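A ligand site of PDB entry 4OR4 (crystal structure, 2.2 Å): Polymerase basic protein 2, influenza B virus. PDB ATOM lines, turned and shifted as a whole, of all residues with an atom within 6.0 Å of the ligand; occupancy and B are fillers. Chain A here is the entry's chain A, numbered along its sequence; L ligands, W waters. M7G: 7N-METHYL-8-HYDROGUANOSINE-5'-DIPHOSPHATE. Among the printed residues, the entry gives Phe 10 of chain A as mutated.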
ATOM      1  N   PHE A  10      37.731 -25.791 -13.824  1.00  0.00           N
ATOM      2  CA  PHE A  10      36.377 -25.683 -14.398  1.00  0.00           C
ATOM      3  C   PHE A  10      35.942 -24.234 -14.362  1.00  0.00           C
ATOM      4  O   PHE A  10      36.598 -23.413 -13.718  1.00  0.00           O
ATOM      5  CB  PHE A  10      35.385 -26.592 -13.674  1.00  0.00           C
ATOM      6  CG  PHE A  10      35.184 -26.234 -12.232  1.00  0.00           C
ATOM      7  CD1 PHE A  10      34.069 -25.475 -11.839  1.00  0.00           C
ATOM      8  CD2 PHE A  10      36.075 -26.673 -11.254  1.00  0.00           C
ATOM      9  CE1 PHE A  10      33.890 -25.115 -10.507  1.00  0.00           C
ATOM     10  CE2 PHE A  10      35.863 -26.343  -9.898  1.00  0.00           C
ATOM     11  CZ  PHE A  10      34.788 -25.561  -9.528  1.00  0.00           C
ATOM     12  N   ARG A  11      34.853 -23.911 -15.052  1.00  0.00           N
ATOM     13  CA  ARG A  11      34.387 -22.509 -15.123  1.00  0.00           C
ATOM     14  C   ARG A  11      33.050 -22.315 -14.432  1.00  0.00           C
ATOM     15  O   ARG A  11      32.224 -23.216 -14.372  1.00  0.00           O
ATOM     16  CB  ARG A  11      34.151 -22.100 -16.602  1.00  0.00           C
ATOM     17  CG  ARG A  11      35.296 -22.475 -17.536  1.00  0.00           C
ATOM     18  CD  ARG A  11      36.592 -21.701 -17.198  1.00  0.00           C
ATOM     19  NE  ARG A  11      36.308 -20.266 -17.272  1.00  0.00           N
ATOM     20  CZ  ARG A  11      36.879 -19.374 -18.086  1.00  0.00           C
ATOM     21  NH1 ARG A  11      37.838 -19.713 -18.908  1.00  0.00           N
ATOM     22  NH2 ARG A  11      36.488 -18.115 -18.022  1.00  0.00           N
ATOM     23  N   PHE A  12      32.849 -21.089 -13.957  1.00  0.00           N
ATOM     24  CA  PHE A  12      31.531 -20.582 -13.650  1.00  0.00           C
ATOM     25  C   PHE A  12      31.436 -19.316 -14.518  1.00  0.00           C
ATOM     26  O   PHE A  12      31.826 -18.249 -14.070  1.00  0.00           O
ATOM     27  CB  PHE A  12      31.455 -20.252 -12.143  1.00  0.00           C
ATOM     28  CG  PHE A  12      30.208 -19.493 -11.723  1.00  0.00           C
ATOM     29  CD1 PHE A  12      28.918 -19.922 -12.137  1.00  0.00           C
ATOM     30  CD2 PHE A  12      30.326 -18.331 -10.908  1.00  0.00           C
ATOM     31  CE1 PHE A  12      27.822 -19.214 -11.744  1.00  0.00           C
ATOM     32  CE2 PHE A  12      29.208 -17.668 -10.460  1.00  0.00           C
ATOM     33  CZ  PHE A  12      27.962 -18.097 -10.871  1.00  0.00           C
ATOM     34  N   LEU A  17      38.052 -21.869 -11.880  1.00  0.00           N
ATOM     35  CA  LEU A  17      38.333 -22.423 -10.542  1.00  0.00           C
ATOM     36  C   LEU A  17      39.120 -23.682 -10.643  1.00  0.00           C
ATOM     37  O   LEU A  17      39.083 -24.379 -11.671  1.00  0.00           O
ATOM     38  CB  LEU A  17      37.030 -22.756  -9.771  1.00  0.00           C
ATOM     39  CG  LEU A  17      36.167 -21.487  -9.657  1.00  0.00           C
ATOM     40  CD1 LEU A  17      35.137 -21.394 -10.774  1.00  0.00           C
ATOM     41  CD2 LEU A  17      35.514 -21.422  -8.305  1.00  0.00           C
ATOM     42  N   ARG A  19      40.014 -26.779  -7.537  1.00  0.00           N
ATOM     43  CA  ARG A  19      39.868 -27.086  -6.133  1.00  0.00           C
ATOM     44  C   ARG A  19      41.247 -27.221  -5.494  1.00  0.00           C
ATOM     45  O   ARG A  19      42.179 -27.819  -6.069  1.00  0.00           O
ATOM     46  CB  ARG A  19      39.062 -28.360  -5.964  1.00  0.00           C
ATOM     47  CG  ARG A  19      38.759 -28.745  -4.530  1.00  0.00           C
ATOM     48  CD  ARG A  19      37.876 -30.004  -4.507  1.00  0.00           C
ATOM     49  NE  ARG A  19      36.700 -29.855  -5.378  1.00  0.00           N
ATOM     50  CZ  ARG A  19      35.567 -29.251  -4.996  1.00  0.00           C
ATOM     51  NH1 ARG A  19      35.442 -28.721  -3.737  1.00  0.00           N
ATOM     52  NH2 ARG A  19      34.585 -29.155  -5.893  1.00  0.00           N
ATOM     53  N   GLY A  24      31.901 -29.794  -1.058  1.00  0.00           N
ATOM     54  CA  GLY A  24      30.614 -29.218  -0.795  1.00  0.00           C
ATOM     55  C   GLY A  24      29.532 -30.240  -1.032  1.00  0.00           C
ATOM     56  O   GLY A  24      29.708 -31.150  -1.820  1.00  0.00           O
ATOM     57  N   LYS A  26      25.332 -30.100  -1.968  1.00  0.00           N
ATOM     58  CA  LYS A  26      24.352 -29.149  -2.383  1.00  0.00           C
ATOM     59  C   LYS A  26      22.945 -29.559  -1.959  1.00  0.00           C
ATOM     60  O   LYS A  26      22.609 -30.710  -2.093  1.00  0.00           O
ATOM     61  CB  LYS A  26      24.397 -29.040  -3.886  1.00  0.00           C
ATOM     62  CG  LYS A  26      23.772 -27.714  -4.327  1.00  0.00           C
ATOM     63  CD  LYS A  26      23.082 -27.860  -5.632  1.00  0.00           C
ATOM     64  CE  LYS A  26      23.992 -28.301  -6.723  1.00  0.00           C
ATOM     65  NZ  LYS A  26      23.031 -28.657  -7.713  1.00  0.00           N
ATOM     66  N   ASP A  28      18.720 -27.946  -2.212  1.00  0.00           N
ATOM     67  CA  ASP A  28      17.876 -26.887  -2.743  1.00  0.00           C
ATOM     68  C   ASP A  28      17.232 -26.109  -1.599  1.00  0.00           C
ATOM     69  O   ASP A  28      16.687 -26.709  -0.662  1.00  0.00           O
ATOM     70  CB  ASP A  28      16.834 -27.416  -3.727  1.00  0.00           C
ATOM     71  CG  ASP A  28      17.363 -27.426  -5.183  1.00  0.00           C
ATOM     72  OD1 ASP A  28      18.542 -27.069  -5.422  1.00  0.00           O
ATOM     73  OD2 ASP A  28      16.606 -27.806  -6.114  1.00  0.00           O
ATOM     74  N   ILE A  41      17.128 -22.228  -5.002  1.00  0.00           N
ATOM     75  CA  ILE A  41      18.509 -22.220  -5.521  1.00  0.00           C
ATOM     76  C   ILE A  41      19.286 -23.360  -4.821  1.00  0.00           C
ATOM     77  O   ILE A  41      19.176 -23.507  -3.620  1.00  0.00           O
ATOM     78  CB  ILE A  41      19.267 -20.878  -5.152  1.00  0.00           C
ATOM     79  CG1 ILE A  41      18.449 -19.620  -5.526  1.00  0.00           C
ATOM     80  CG2 ILE A  41      20.689 -20.864  -5.764  1.00  0.00           C
ATOM     81  CD1 ILE A  41      19.251 -18.347  -5.641  1.00  0.00           C
ATOM     82  N   GLY A  42      20.090 -24.103  -5.576  1.00  0.00           N
ATOM     83  CA  GLY A  42      21.067 -25.060  -4.981  1.00  0.00           C
ATOM     84  C   GLY A  42      22.106 -24.363  -4.142  1.00  0.00           C
ATOM     85  O   GLY A  42      23.008 -23.637  -4.668  1.00  0.00           O
ATOM     86  N   TRP A  44      25.237 -24.664  -1.611  1.00  0.00           N
ATOM     87  CA  TRP A  44      26.334 -25.545  -1.174  1.00  0.00           C
ATOM     88  C   TRP A  44      26.641 -25.446   0.334  1.00  0.00           C
ATOM     89  O   TRP A  44      26.723 -24.360   0.902  1.00  0.00           O
ATOM     90  CB  TRP A  44      27.630 -25.274  -1.961  1.00  0.00           C
ATOM     91  CG  TRP A  44      27.533 -25.653  -3.411  1.00  0.00           C
ATOM     92  CD1 TRP A  44      27.171 -24.842  -4.450  1.00  0.00           C
ATOM     93  CD2 TRP A  44      27.716 -26.970  -3.954  1.00  0.00           C
ATOM     94  NE1 TRP A  44      27.138 -25.558  -5.610  1.00  0.00           N
ATOM     95  CE2 TRP A  44      27.476 -26.862  -5.359  1.00  0.00           C
ATOM     96  CE3 TRP A  44      28.049 -28.235  -3.397  1.00  0.00           C
ATOM     97  CZ2 TRP A  44      27.547 -27.959  -6.227  1.00  0.00           C
ATOM     98  CZ3 TRP A  44      28.139 -29.369  -4.270  1.00  0.00           C
ATOM     99  CH2 TRP A  44      27.901 -29.204  -5.678  1.00  0.00           C
ATOM    100  N   GLU A  48      35.031 -24.991   1.463  1.00  0.00           N
ATOM    101  CA  GLU A  48      35.726 -25.367   0.241  1.00  0.00           C
ATOM    102  C   GLU A  48      36.750 -24.282  -0.092  1.00  0.00           C
ATOM    103  O   GLU A  48      36.547 -23.108   0.196  1.00  0.00           O
ATOM    104  CB  GLU A  48      34.725 -25.524  -0.915  1.00  0.00           C
ATOM    105  CG  GLU A  48      33.732 -26.718  -0.844  1.00  0.00           C
ATOM    106  CD  GLU A  48      32.760 -26.657  -2.028  1.00  0.00           C
ATOM    107  OE1 GLU A  48      31.773 -25.891  -1.956  1.00  0.00           O
ATOM    108  OE2 GLU A  48      33.002 -27.326  -3.077  1.00  0.00           O
ATOM    109  N   PHE A  50      39.495 -22.804  -3.267  1.00  0.00           N
ATOM    110  CA  PHE A  50      39.794 -22.851  -4.710  1.00  0.00           C
ATOM    111  C   PHE A  50      40.833 -21.839  -5.133  1.00  0.00           C
ATOM    112  O   PHE A  50      40.776 -20.699  -4.709  1.00  0.00           O
ATOM    113  CB  PHE A  50      38.563 -22.545  -5.535  1.00  0.00           C
ATOM    114  CG  PHE A  50      37.369 -23.452  -5.285  1.00  0.00           C
ATOM    115  CD1 PHE A  50      37.202 -24.641  -6.009  1.00  0.00           C
ATOM    116  CD2 PHE A  50      36.360 -23.086  -4.355  1.00  0.00           C
ATOM    117  CE1 PHE A  50      36.036 -25.481  -5.781  1.00  0.00           C
ATOM    118  CE2 PHE A  50      35.240 -23.883  -4.125  1.00  0.00           C
ATOM    119  CZ  PHE A  50      35.050 -25.080  -4.853  1.00  0.00           C
ATOM    120  N   LYS A  63      35.215 -20.579   0.965  1.00  0.00           N
ATOM    121  CA  LYS A  63      33.809 -20.336   1.229  1.00  0.00           C
ATOM    122  C   LYS A  63      33.301 -21.381   2.194  1.00  0.00           C
ATOM    123  O   LYS A  63      33.902 -22.416   2.338  1.00  0.00           O
ATOM    124  CB  LYS A  63      32.986 -20.402  -0.080  1.00  0.00           C
ATOM    125  CG  LYS A  63      32.821 -21.825  -0.601  1.00  0.00           C
ATOM    126  CD  LYS A  63      31.890 -21.931  -1.783  1.00  0.00           C
ATOM    127  CE  LYS A  63      30.415 -21.478  -1.526  1.00  0.00           C
ATOM    128  NZ  LYS A  63      29.617 -22.214  -0.474  1.00  0.00           N
ATOM    129  N   PHE A  91      29.766 -16.619  -6.538  1.00  0.00           N
ATOM    130  CA  PHE A  91      30.056 -18.058  -6.391  1.00  0.00           C
ATOM    131  C   PHE A  91      30.029 -18.469  -4.933  1.00  0.00           C
ATOM    132  O   PHE A  91      29.657 -19.564  -4.695  1.00  0.00           O
ATOM    133  CB  PHE A  91      31.436 -18.411  -6.958  1.00  0.00           C
ATOM    134  CG  PHE A  91      31.769 -19.897  -6.913  1.00  0.00           C
ATOM    135  CD1 PHE A  91      31.393 -20.751  -7.971  1.00  0.00           C
ATOM    136  CD2 PHE A  91      32.503 -20.450  -5.813  1.00  0.00           C
ATOM    137  CE1 PHE A  91      31.735 -22.121  -7.956  1.00  0.00           C
ATOM    138  CE2 PHE A  91      32.850 -21.826  -5.765  1.00  0.00           C
ATOM    139  CZ  PHE A  91      32.464 -22.692  -6.840  1.00  0.00           C
ATOM    140  N   GLN A  93      27.962 -17.599  -2.719  1.00  0.00           N
ATOM    141  CA  GLN A  93      26.545 -17.676  -2.333  1.00  0.00           C
ATOM    142  C   GLN A  93      26.309 -16.943  -0.998  1.00  0.00           C
ATOM    143  O   GLN A  93      25.401 -17.249  -0.248  1.00  0.00           O
ATOM    144  CB  GLN A  93      26.061 -19.119  -2.240  1.00  0.00           C
ATOM    145  CG  GLN A  93      26.173 -19.845  -3.585  1.00  0.00           C
ATOM    146  CD  GLN A  93      25.587 -21.207  -3.523  1.00  0.00           C
ATOM    147  OE1 GLN A  93      25.859 -21.999  -2.586  1.00  0.00           O
ATOM    148  NE2 GLN A  93      24.800 -21.553  -4.550  1.00  0.00           N
ATOM    149  N   SER A 116      19.729 -20.872 -15.281  1.00  0.00           N
ATOM    150  CA  SER A 116      20.478 -21.144 -14.074  1.00  0.00           C
ATOM    151  C   SER A 116      20.394 -19.971 -13.107  1.00  0.00           C
ATOM    152  O   SER A 116      20.773 -18.849 -13.467  1.00  0.00           O
ATOM    153  CB  SER A 116      21.920 -21.454 -14.433  1.00  0.00           C
ATOM    154  OG  SER A 116      22.752 -21.333 -13.286  1.00  0.00           O
ATOM    155  N   PRO A 117      19.813 -20.190 -11.899  1.00  0.00           N
ATOM    156  CA  PRO A 117      19.787 -19.036 -11.001  1.00  0.00           C
ATOM    157  C   PRO A 117      21.184 -18.418 -10.729  1.00  0.00           C
ATOM    158  O   PRO A 117      21.344 -17.179 -10.718  1.00  0.00           O
ATOM    159  CB  PRO A 117      19.156 -19.573  -9.727  1.00  0.00           C
ATOM    160  CG  PRO A 117      18.305 -20.788 -10.172  1.00  0.00           C
ATOM    161  CD  PRO A 117      19.050 -21.350 -11.379  1.00  0.00           C
ATOM    162  N   MET A 118      22.182 -19.253 -10.525  1.00  0.00           N
ATOM    163  CA  MET A 118      23.528 -18.779 -10.249  1.00  0.00           C
ATOM    164  C   MET A 118      24.158 -18.031 -11.438  1.00  0.00           C
ATOM    165  O   MET A 118      24.827 -16.990 -11.260  1.00  0.00           O
ATOM    166  CB  MET A 118      24.442 -19.925  -9.742  1.00  0.00           C
ATOM    167  CG  MET A 118      24.098 -20.388  -8.271  1.00  0.00           C
ATOM    168  SD  MET A 118      24.524 -19.066  -7.085  1.00  0.00           S
ATOM    169  CE  MET A 118      26.278 -18.994  -7.358  1.00  0.00           C
ATOM    170  N   TYR A 119      23.994 -18.557 -12.661  1.00  0.00           N
ATOM    171  CA  TYR A 119      24.529 -17.871 -13.838  1.00  0.00           C
ATOM    172  C   TYR A 119      23.831 -16.519 -14.061  1.00  0.00           C
ATOM    173  O   TYR A 119      24.476 -15.502 -14.396  1.00  0.00           O
ATOM    174  CB  TYR A 119      24.432 -18.800 -15.039  1.00  0.00           C
ATOM    175  CG  TYR A 119      25.507 -19.874 -14.969  1.00  0.00           C
ATOM    176  CD1 TYR A 119      26.765 -19.594 -15.457  1.00  0.00           C
ATOM    177  CD2 TYR A 119      25.276 -21.132 -14.385  1.00  0.00           C
ATOM    178  CE1 TYR A 119      27.749 -20.521 -15.416  1.00  0.00           C
ATOM    179  CE2 TYR A 119      26.273 -22.087 -14.340  1.00  0.00           C
ATOM    180  CZ  TYR A 119      27.515 -21.743 -14.861  1.00  0.00           C
ATOM    181  OH  TYR A 119      28.592 -22.573 -14.894  1.00  0.00           O
HETATM  182  PA  M7G L   1      23.639 -24.586 -11.609  1.00  0.00           P
HETATM  183  O1A M7G L   1      22.426 -23.724 -11.892  1.00  0.00           O
HETATM  184  O2A M7G L   1      24.679 -24.789 -12.616  1.00  0.00           O
HETATM  185  O3A M7G L   1      23.089 -26.107 -11.305  1.00  0.00           O
HETATM  186  O5' M7G L   1      24.376 -24.170 -10.212  1.00  0.00           O
HETATM  187  PB  M7G L   1      21.912 -26.443 -10.244  1.00  0.00           P
HETATM  188  O1B M7G L   1      20.673 -25.602 -10.233  1.00  0.00           O
HETATM  189  O2B M7G L   1      21.646 -27.918 -10.480  1.00  0.00           O
HETATM  190  O3B M7G L   1      22.324 -26.257  -8.704  1.00  0.00           O
HETATM  191  C5' M7G L   1      25.561 -24.876  -9.856  1.00  0.00           C
HETATM  192  C4' M7G L   1      26.443 -23.863  -9.105  1.00  0.00           C
HETATM  193  O4' M7G L   1      27.357 -24.621  -8.295  1.00  0.00           O
HETATM  194  C3' M7G L   1      27.273 -23.125 -10.144  1.00  0.00           C
HETATM  195  O3' M7G L   1      27.570 -21.851  -9.602  1.00  0.00           O
HETATM  196  C2' M7G L   1      28.536 -23.944 -10.185  1.00  0.00           C
HETATM  197  O2' M7G L   1      29.644 -23.065 -10.464  1.00  0.00           O
HETATM  198  C1' M7G L   1      28.705 -24.488  -8.754  1.00  0.00           C
HETATM  199  N9  M7G L   1      29.675 -25.635  -8.720  1.00  0.00           N
HETATM  200  C8  M7G L   1      29.708 -26.994  -9.443  1.00  0.00           C
HETATM  201  N7  M7G L   1      30.771 -27.924  -8.819  1.00  0.00           N
HETATM  202  CM7 M7G L   1      30.858 -29.086  -9.423  1.00  0.00           C
HETATM  203  C5  M7G L   1      30.890 -27.259  -7.569  1.00  0.00           C
HETATM  204  C6  M7G L   1      31.507 -27.624  -6.303  1.00  0.00           C
HETATM  205  O6  M7G L   1      32.066 -28.691  -6.258  1.00  0.00           O
HETATM  206  N1  M7G L   1      31.418 -26.767  -5.226  1.00  0.00           N
HETATM  207  C2  M7G L   1      30.818 -25.533  -5.271  1.00  0.00           C
HETATM  208  N2  M7G L   1      30.741 -24.679  -4.206  1.00  0.00           N
HETATM  209  N3  M7G L   1      30.205 -25.130  -6.411  1.00  0.00           N
HETATM  210  C4  M7G L   1      30.200 -25.952  -7.499  1.00  0.00           C
HETATM  211  O   HOH W   1      21.653 -22.169  -9.675  1.00  0.00           O
HETATM  212  O   HOH W   2      20.039 -23.792  -8.274  1.00  0.00           O
HETATM  213  O   HOH W   3      29.230 -22.168  -5.410  1.00  0.00           O
HETATM  214  O   HOH W   4      23.016 -23.623  -7.504  1.00  0.00           O
HETATM  215  O   HOH W   5      31.904 -30.244  -3.738  1.00  0.00           O
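NH2 of Arg 19 sits at hydrogen-bond distance from O6 of the ligand, 2.6 Å away. An oxygen (O3B) of the ligand lies within salt-bridge range of the side-chain amino group (NZ) of Lys 26, 2.7 Å away. A nitrogen (N1) of the ligand sits at hydrogen-bond distance from the side-chain carboxylate (OE2) of Glu 48 (2.7 Å). OG of Ser 116 sits at hydrogen-bond distance from O1A of the ligand (2.8 Å). The indole nitrogen of Trp 44 lies within hydrogen-bond range of an oxygen (O4') of the ligand, 2.9 Å away.
The guanidinium group (NH1) of Arg 19 is in salt-bridge range of the side-chain carboxylate (OE2) of Glu 48. The backbone NH (N) of Glu 48 lies within hydrogen-bond range of the backbone carbonyl oxygen (O) of Lys 63, at 2.9 Å. OE2 of Glu 48 sits at hydrogen-bond distance from N of Gly 24 (3.4 Å). N of Tyr 119 lies close to OG of Ser 116 (3.1 Å). The side-chain amide oxygen (OE1) of Gln 93 sits at hydrogen-bond distance from the backbone NH (N) of Trp 44 (2.9 Å). The side-chain sulfur (SD) of Met 118 sits at hydrogen-bond distance from the side-chain amide nitrogen (NE2) of Gln 93 (3.6 Å).
Phe 12 touches the ligand (CE1 to O3', 3.4 Å). CD of Lys 63 touches N2 of the ligand (3.8 Å). Phe 91 touches the ligand. Met 118 touches the ligand. Tyr 119 touches the ligand. Within 4 Å of the ligand: Phe 12, Arg 19, Lys 26, Trp 44, Glu 48, Lys 63, Phe 91, Ser 116, Met 118 and Tyr 119.
Water W2 bridges the backbone NH of Gly 42 (2.7 Å) and an oxygen (O1B) of the ligand (2.7 Å). Water W1 lies within hydrogen-bond range of O1A of the ligand (2.8 Å) and N of Met 118 (3.1 Å). Water W5 lies within hydrogen-bond range of the backbone NH (N) of Gly 24, an oxygen (O6) of the ligand and the side-chain carboxylate (OE2) of Glu 48. Water W4 lies within hydrogen-bond range of the backbone carbonyl oxygen (O) of Gly 42 and an oxygen (O3B) of the ligand. Water W3 lies within hydrogen-bond range of O of Phe 91 and N2 of the ligand.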
